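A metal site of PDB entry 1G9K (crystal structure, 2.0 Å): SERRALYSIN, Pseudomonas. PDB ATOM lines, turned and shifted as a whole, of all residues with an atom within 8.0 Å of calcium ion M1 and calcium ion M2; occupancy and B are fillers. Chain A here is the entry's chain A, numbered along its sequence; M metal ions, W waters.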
ATOM      1  N   GLU A 248     -33.720   0.761   1.547  1.00  0.00           N
ATOM      2  CA  GLU A 248     -32.754   0.012   0.749  1.00  0.00           C
ATOM      3  C   GLU A 248     -31.389  -0.069   1.428  1.00  0.00           C
ATOM      4  O   GLU A 248     -30.598  -0.975   1.160  1.00  0.00           O
ATOM      5  CB  GLU A 248     -32.591   0.696  -0.596  1.00  0.00           C
ATOM      6  CG  GLU A 248     -33.898   1.040  -1.288  1.00  0.00           C
ATOM      7  CD  GLU A 248     -34.333  -0.012  -2.286  1.00  0.00           C
ATOM      8  OE1 GLU A 248     -34.568  -1.168  -1.870  1.00  0.00           O
ATOM      9  OE2 GLU A 248     -34.415   0.324  -3.479  1.00  0.00           O
ATOM     10  N   THR A 249     -31.128   0.872   2.328  1.00  0.00           N
ATOM     11  CA  THR A 249     -29.855   0.963   3.013  1.00  0.00           C
ATOM     12  C   THR A 249     -29.527  -0.151   4.016  1.00  0.00           C
ATOM     13  O   THR A 249     -30.279  -0.397   4.959  1.00  0.00           O
ATOM     14  CB  THR A 249     -29.743   2.316   3.742  1.00  0.00           C
ATOM     15  OG1 THR A 249     -29.977   3.363   2.795  1.00  0.00           O
ATOM     16  CG2 THR A 249     -28.364   2.492   4.343  1.00  0.00           C
ATOM     17  N   ARG A 250     -28.380  -0.805   3.803  1.00  0.00           N
ATOM     18  CA  ARG A 250     -27.939  -1.881   4.675  1.00  0.00           C
ATOM     19  C   ARG A 250     -29.091  -2.858   4.951  1.00  0.00           C
ATOM     20  O   ARG A 250     -29.296  -3.277   6.085  1.00  0.00           O
ATOM     21  CB  ARG A 250     -27.394  -1.273   5.979  1.00  0.00           C
ATOM     22  CG  ARG A 250     -26.146  -0.367   5.767  1.00  0.00           C
ATOM     23  CD  ARG A 250     -25.595   0.204   7.074  1.00  0.00           C
ATOM     24  NE  ARG A 250     -26.399   1.293   7.603  1.00  0.00           N
ATOM     25  CZ  ARG A 250     -26.318   2.565   7.219  1.00  0.00           C
ATOM     26  NH1 ARG A 250     -25.450   2.920   6.281  1.00  0.00           N
ATOM     27  NH2 ARG A 250     -27.107   3.487   7.764  1.00  0.00           N
ATOM     28  N   ALA A 251     -29.835  -3.212   3.910  1.00  0.00           N
ATOM     29  CA  ALA A 251     -30.976  -4.109   4.034  1.00  0.00           C
ATOM     30  C   ALA A 251     -30.625  -5.578   4.321  1.00  0.00           C
ATOM     31  O   ALA A 251     -31.513  -6.391   4.542  1.00  0.00           O
ATOM     32  CB  ALA A 251     -31.844  -4.024   2.776  1.00  0.00           C
ATOM     33  N   ASP A 252     -29.331  -5.900   4.318  1.00  0.00           N
ATOM     34  CA  ASP A 252     -28.867  -7.255   4.601  1.00  0.00           C
ATOM     35  C   ASP A 252     -28.289  -7.277   6.018  1.00  0.00           C
ATOM     36  O   ASP A 252     -28.324  -6.274   6.718  1.00  0.00           O
ATOM     37  CB  ASP A 252     -27.802  -7.679   3.592  1.00  0.00           C
ATOM     38  CG  ASP A 252     -26.666  -6.677   3.486  1.00  0.00           C
ATOM     39  OD1 ASP A 252     -25.631  -7.011   2.873  1.00  0.00           O
ATOM     40  OD2 ASP A 252     -26.802  -5.551   4.013  1.00  0.00           O
ATOM     41  N   ASP A 253     -27.765  -8.432   6.448  1.00  0.00           N
ATOM     42  CA  ASP A 253     -27.183  -8.552   7.782  1.00  0.00           C
ATOM     43  C   ASP A 253     -26.064  -7.537   7.966  1.00  0.00           C
ATOM     44  O   ASP A 253     -25.121  -7.487   7.171  1.00  0.00           O
ATOM     45  CB  ASP A 253     -26.635  -9.972   8.000  1.00  0.00           C
ATOM     46  CG  ASP A 253     -27.708 -11.042   7.985  1.00  0.00           C
ATOM     47  OD1 ASP A 253     -28.900 -10.687   7.800  1.00  0.00           O
ATOM     48  OD2 ASP A 253     -27.368 -12.229   8.154  1.00  0.00           O
ATOM     49  N   THR A 254     -26.168  -6.728   9.017  1.00  0.00           N
ATOM     50  CA  THR A 254     -25.168  -5.680   9.255  1.00  0.00           C
ATOM     51  C   THR A 254     -24.609  -5.674  10.665  1.00  0.00           C
ATOM     52  O   THR A 254     -25.326  -5.913  11.629  1.00  0.00           O
ATOM     53  CB  THR A 254     -25.770  -4.292   8.983  1.00  0.00           C
ATOM     54  OG1 THR A 254     -26.635  -4.362   7.840  1.00  0.00           O
ATOM     55  CG2 THR A 254     -24.666  -3.283   8.706  1.00  0.00           C
ATOM     56  N   VAL A 255     -23.316  -5.380  10.786  1.00  0.00           N
ATOM     57  CA  VAL A 255     -22.677  -5.291  12.081  1.00  0.00           C
ATOM     58  C   VAL A 255     -22.196  -3.848  12.267  1.00  0.00           C
ATOM     59  O   VAL A 255     -21.584  -3.280  11.366  1.00  0.00           O
ATOM     60  CB  VAL A 255     -21.461  -6.249  12.203  1.00  0.00           C
ATOM     61  CG1 VAL A 255     -20.853  -6.131  13.594  1.00  0.00           C
ATOM     62  CG2 VAL A 255     -21.896  -7.686  11.935  1.00  0.00           C
ATOM     63  N   TYR A 256     -22.510  -3.257  13.418  1.00  0.00           N
ATOM     64  CA  TYR A 256     -22.103  -1.887  13.745  1.00  0.00           C
ATOM     65  C   TYR A 256     -21.159  -1.937  14.944  1.00  0.00           C
ATOM     66  O   TYR A 256     -21.300  -2.802  15.805  1.00  0.00           O
ATOM     67  CB  TYR A 256     -23.321  -1.020  14.107  1.00  0.00           C
ATOM     68  CG  TYR A 256     -24.350  -0.900  13.010  1.00  0.00           C
ATOM     69  CD1 TYR A 256     -25.298  -1.903  12.799  1.00  0.00           C
ATOM     70  CD2 TYR A 256     -24.338   0.195  12.145  1.00  0.00           C
ATOM     71  CE1 TYR A 256     -26.213  -1.821  11.736  1.00  0.00           C
ATOM     72  CE2 TYR A 256     -25.238   0.289  11.097  1.00  0.00           C
ATOM     73  CZ  TYR A 256     -26.166  -0.720  10.891  1.00  0.00           C
ATOM     74  OH  TYR A 256     -27.028  -0.626   9.827  1.00  0.00           O
ATOM     75  N   THR A 261     -19.540  -3.854   9.493  1.00  0.00           N
ATOM     76  CA  THR A 261     -19.704  -4.172   8.079  1.00  0.00           C
ATOM     77  C   THR A 261     -20.605  -3.118   7.448  1.00  0.00           C
ATOM     78  O   THR A 261     -21.097  -3.285   6.330  1.00  0.00           O
ATOM     79  CB  THR A 261     -20.338  -5.559   7.862  1.00  0.00           C
ATOM     80  OG1 THR A 261     -21.629  -5.608   8.490  1.00  0.00           O
ATOM     81  CG2 THR A 261     -19.459  -6.649   8.457  1.00  0.00           C
ATOM     82  N   VAL A 280     -28.379   4.569  14.767  1.00  0.00           N
ATOM     83  CA  VAL A 280     -28.455   3.493  13.788  1.00  0.00           C
ATOM     84  C   VAL A 280     -29.676   3.525  12.865  1.00  0.00           C
ATOM     85  O   VAL A 280     -30.813   3.568  13.326  1.00  0.00           O
ATOM     86  CB  VAL A 280     -28.424   2.110  14.507  1.00  0.00           C
ATOM     87  CG1 VAL A 280     -28.504   0.979  13.480  1.00  0.00           C
ATOM     88  CG2 VAL A 280     -27.159   1.981  15.332  1.00  0.00           C
ATOM     89  N   TRP A 281     -29.426   3.535  11.558  1.00  0.00           N
ATOM     90  CA  TRP A 281     -30.505   3.461  10.586  1.00  0.00           C
ATOM     91  C   TRP A 281     -30.148   2.218   9.782  1.00  0.00           C
ATOM     92  O   TRP A 281     -29.022   2.077   9.319  1.00  0.00           O
ATOM     93  CB  TRP A 281     -30.582   4.677   9.667  1.00  0.00           C
ATOM     94  CG  TRP A 281     -31.538   4.436   8.519  1.00  0.00           C
ATOM     95  CD1 TRP A 281     -31.202   4.221   7.202  1.00  0.00           C
ATOM     96  CD2 TRP A 281     -32.948   4.201   8.611  1.00  0.00           C
ATOM     97  NE1 TRP A 281     -32.315   3.865   6.489  1.00  0.00           N
ATOM     98  CE2 TRP A 281     -33.401   3.850   7.319  1.00  0.00           C
ATOM     99  CE3 TRP A 281     -33.882   4.253   9.667  1.00  0.00           C
ATOM    100  CZ2 TRP A 281     -34.743   3.544   7.053  1.00  0.00           C
ATOM    101  CZ3 TRP A 281     -35.223   3.960   9.396  1.00  0.00           C
ATOM    102  CH2 TRP A 281     -35.637   3.604   8.097  1.00  0.00           C
ATOM    103  N   ASP A 282     -31.115   1.313   9.633  1.00  0.00           N
ATOM    104  CA  ASP A 282     -30.906   0.057   8.921  1.00  0.00           C
ATOM    105  C   ASP A 282     -32.206  -0.377   8.238  1.00  0.00           C
ATOM    106  O   ASP A 282     -33.284  -0.279   8.821  1.00  0.00           O
ATOM    107  CB  ASP A 282     -30.453  -0.993   9.950  1.00  0.00           C
ATOM    108  CG  ASP A 282     -30.001  -2.296   9.307  1.00  0.00           C
ATOM    109  OD1 ASP A 282     -30.856  -3.034   8.776  1.00  0.00           O
ATOM    110  OD2 ASP A 282     -28.787  -2.559   9.333  1.00  0.00           O
ATOM    111  N   GLY A 283     -32.099  -0.841   6.998  1.00  0.00           N
ATOM    112  CA  GLY A 283     -33.275  -1.232   6.242  1.00  0.00           C
ATOM    113  C   GLY A 283     -33.850  -2.631   6.460  1.00  0.00           C
ATOM    114  O   GLY A 283     -35.013  -2.877   6.133  1.00  0.00           O
ATOM    115  N   GLY A 284     -33.042  -3.535   6.999  1.00  0.00           N
ATOM    116  CA  GLY A 284     -33.539  -4.888   7.229  1.00  0.00           C
ATOM    117  C   GLY A 284     -32.421  -5.887   7.455  1.00  0.00           C
ATOM    118  O   GLY A 284     -31.240  -5.523   7.424  1.00  0.00           O
ATOM    119  N   GLY A 285     -32.794  -7.141   7.685  1.00  0.00           N
ATOM    120  CA  GLY A 285     -31.815  -8.188   7.906  1.00  0.00           C
ATOM    121  C   GLY A 285     -31.567  -8.494   9.372  1.00  0.00           C
ATOM    122  O   GLY A 285     -32.210  -7.925  10.252  1.00  0.00           O
ATOM    123  N   ASN A 286     -30.637  -9.404   9.633  1.00  0.00           N
ATOM    124  CA  ASN A 286     -30.284  -9.796  10.999  1.00  0.00           C
ATOM    125  C   ASN A 286     -29.043  -8.973  11.353  1.00  0.00           C
ATOM    126  O   ASN A 286     -27.947  -9.251  10.860  1.00  0.00           O
ATOM    127  CB  ASN A 286     -29.964 -11.285  11.078  1.00  0.00           C
ATOM    128  CG  ASN A 286     -29.742 -11.756  12.500  1.00  0.00           C
ATOM    129  OD1 ASN A 286     -30.692 -11.854  13.283  1.00  0.00           O
ATOM    130  ND2 ASN A 286     -28.503 -12.035  12.840  1.00  0.00           N
ATOM    131  N   ASP A 287     -29.232  -7.998  12.227  1.00  0.00           N
ATOM    132  CA  ASP A 287     -28.178  -7.060  12.606  1.00  0.00           C
ATOM    133  C   ASP A 287     -27.649  -7.154  14.027  1.00  0.00           C
ATOM    134  O   ASP A 287     -28.369  -7.529  14.947  1.00  0.00           O
ATOM    135  CB  ASP A 287     -28.697  -5.654  12.332  1.00  0.00           C
ATOM    136  CG  ASP A 287     -29.471  -5.598  11.048  1.00  0.00           C
ATOM    137  OD1 ASP A 287     -28.864  -5.817   9.986  1.00  0.00           O
ATOM    138  OD2 ASP A 287     -30.702  -5.344  11.098  1.00  0.00           O
ATOM    139  N   THR A 288     -26.376  -6.771  14.206  1.00  0.00           N
ATOM    140  CA  THR A 288     -25.742  -6.843  15.512  1.00  0.00           C
ATOM    141  C   THR A 288     -24.976  -5.577  15.910  1.00  0.00           C
ATOM    142  O   THR A 288     -24.342  -4.934  15.077  1.00  0.00           O
ATOM    143  CB  THR A 288     -24.770  -8.033  15.563  1.00  0.00           C
ATOM    144  OG1 THR A 288     -25.412  -9.195  15.009  1.00  0.00           O
ATOM    145  CG2 THR A 288     -24.363  -8.321  16.995  1.00  0.00           C
ATOM    146  N   VAL A 323     -36.684   0.951  13.303  1.00  0.00           N
ATOM    147  CA  VAL A 323     -35.579   0.030  13.031  1.00  0.00           C
ATOM    148  C   VAL A 323     -35.524  -1.095  14.053  1.00  0.00           C
ATOM    149  O   VAL A 323     -35.645  -0.865  15.248  1.00  0.00           O
ATOM    150  CB  VAL A 323     -34.226   0.782  13.033  1.00  0.00           C
ATOM    151  CG1 VAL A 323     -33.083  -0.204  12.836  1.00  0.00           C
ATOM    152  CG2 VAL A 323     -34.209   1.834  11.943  1.00  0.00           C
ATOM    153  N   THR A 324     -35.353  -2.324  13.562  1.00  0.00           N
ATOM    154  CA  THR A 324     -35.254  -3.475  14.453  1.00  0.00           C
ATOM    155  C   THR A 324     -33.860  -4.079  14.388  1.00  0.00           C
ATOM    156  O   THR A 324     -33.457  -4.618  13.353  1.00  0.00           O
ATOM    157  CB  THR A 324     -36.282  -4.586  14.098  1.00  0.00           C
ATOM    158  OG1 THR A 324     -37.610  -4.040  14.114  1.00  0.00           O
ATOM    159  CG2 THR A 324     -36.201  -5.719  15.101  1.00  0.00           C
ATOM    160  N   ILE A 325     -33.112  -3.962  15.481  1.00  0.00           N
ATOM    161  CA  ILE A 325     -31.761  -4.516  15.593  1.00  0.00           C
ATOM    162  C   ILE A 325     -31.921  -5.781  16.428  1.00  0.00           C
ATOM    163  O   ILE A 325     -32.456  -5.734  17.542  1.00  0.00           O
ATOM    164  CB  ILE A 325     -30.797  -3.555  16.298  1.00  0.00           C
ATOM    165  CG1 ILE A 325     -30.764  -2.211  15.563  1.00  0.00           C
ATOM    166  CG2 ILE A 325     -29.390  -4.166  16.363  1.00  0.00           C
ATOM    167  CD1 ILE A 325     -30.341  -2.323  14.106  1.00  0.00           C
ATOM    168  N   GLU A 326     -31.426  -6.887  15.898  1.00  0.00           N
ATOM    169  CA  GLU A 326     -31.553  -8.192  16.542  1.00  0.00           C
ATOM    170  C   GLU A 326     -30.561  -8.610  17.620  1.00  0.00           C
ATOM    171  O   GLU A 326     -30.949  -9.198  18.638  1.00  0.00           O
ATOM    172  CB  GLU A 326     -31.558  -9.292  15.464  1.00  0.00           C
ATOM    173  CG  GLU A 326     -32.747  -9.273  14.507  1.00  0.00           C
ATOM    174  CD  GLU A 326     -32.783  -8.066  13.590  1.00  0.00           C
ATOM    175  OE1 GLU A 326     -31.718  -7.504  13.255  1.00  0.00           O
ATOM    176  OE2 GLU A 326     -33.898  -7.671  13.190  1.00  0.00           O
ATOM    177  N   ASN A 327     -29.280  -8.324  17.402  1.00  0.00           N
ATOM    178  CA  ASN A 327     -28.252  -8.754  18.346  1.00  0.00           C
ATOM    179  C   ASN A 327     -27.358  -7.667  18.931  1.00  0.00           C
ATOM    180  O   ASN A 327     -27.193  -6.603  18.356  1.00  0.00           O
ATOM    181  CB  ASN A 327     -27.368  -9.806  17.680  1.00  0.00           C
ATOM    182  CG  ASN A 327     -28.141 -10.729  16.766  1.00  0.00           C
ATOM    183  OD1 ASN A 327     -29.153 -11.313  17.173  1.00  0.00           O
ATOM    184  ND2 ASN A 327     -27.672 -10.885  15.529  1.00  0.00           N
ATOM    185  N   ASN A 340     -35.334  -6.803  22.577  1.00  0.00           N
ATOM    186  CA  ASN A 340     -36.649  -6.310  22.195  1.00  0.00           C
ATOM    187  C   ASN A 340     -37.602  -7.489  21.954  1.00  0.00           C
ATOM    188  O   ASN A 340     -37.293  -8.627  22.319  1.00  0.00           O
ATOM    189  CB  ASN A 340     -36.543  -5.452  20.931  1.00  0.00           C
ATOM    190  CG  ASN A 340     -35.675  -6.077  19.860  1.00  0.00           C
ATOM    191  OD1 ASN A 340     -35.767  -7.275  19.586  1.00  0.00           O
ATOM    192  ND2 ASN A 340     -34.820  -5.262  19.239  1.00  0.00           N
ATOM    193  N   ALA A 342     -38.228  -9.041  19.344  1.00  0.00           N
ATOM    194  CA  ALA A 342     -37.736 -10.015  18.386  1.00  0.00           C
ATOM    195  C   ALA A 342     -36.803 -11.013  19.052  1.00  0.00           C
ATOM    196  O   ALA A 342     -36.394 -10.823  20.202  1.00  0.00           O
ATOM    197  CB  ALA A 342     -37.030  -9.298  17.243  1.00  0.00           C
HETATM  198 CA    CA M   1     -29.097  -4.590   8.050  1.00  0.00          CA
HETATM  199 CA    CA M   2     -32.851  -6.049  11.572  1.00  0.00          CA
HETATM  200  O   HOH W   1     -32.980  -4.004  10.316  1.00  0.00           O
HETATM  201  O   HOH W   2     -35.256  -6.241  10.525  1.00  0.00           O
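O of Ala 251 is in hydrogen-bond range of N of Gly 285 (3.5 Å).
The backbone carbonyl oxygen of Thr 254 is in hydrogen-bond range of the backbone NH of Thr 288 (2.9 Å).
The side-chain hydroxyl (OH) of Tyr 256 is in hydrogen-bond range of the guanidinium group (NE) of Arg 250, at 3.0 Å.
The side-chain carboxylate of Asp 282 sits close to the side-chain hydroxyl of Tyr 256, 2.7 Å away.
The backbone carbonyl oxygen (O) of Asp 287 lies within hydrogen-bond range of the backbone NH (N) of Asn 327 (2.7 Å).
The backbone carbonyl oxygen of Trp 281 is in hydrogen-bond range of the guanidinium group of Arg 250.
Of the 26 residues printed, 6 come within 4 Å of calcium ion M1.
The nearest printed residue that does not touch calcium ion M1 is Ala 251 (4.1 Å).
Within 4 Å of calcium ion M2: Gly 285, Asp 287, Thr 324 and Glu 326.
The nearest printed residue that does not touch calcium ion M2 is Gly 284 (4.1 Å).
O of Asp 252 is bound to calcium ion M1, at 2.3 Å.
Calcium ion M1 is bound by the side-chain carboxylate (OD1) of Asp 287, 2.3 Å away.
Calcium ion M1 is bound by O of Arg 250 (2.4 Å).
O of Gly 284 is bound to calcium ion M1 (2.4 Å).
The side-chain carboxylate (OD2) of Asp 282 binds calcium ion M1 (2.4 Å).
OD1 of Asp 282 binds calcium ion M1.
Calcium ion M1 is bound by OG1 of Thr 254 (2.5 Å).
Calcium ion M2 is bound by the side-chain carboxylate (OD2) of Asp 287 (2.3 Å), the backbone carbonyl oxygen (O) of Thr 324 (2.4 Å), the backbone carbonyl oxygen (O) of Gly 285 (2.4 Å), water W1 (2.4 Å), the side-chain carboxylate (OE1) of Glu 326 (2.5 Å), the side-chain carboxylate (OE2) of Glu 326 (2.5 Å) and water W2 (2.6 Å).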
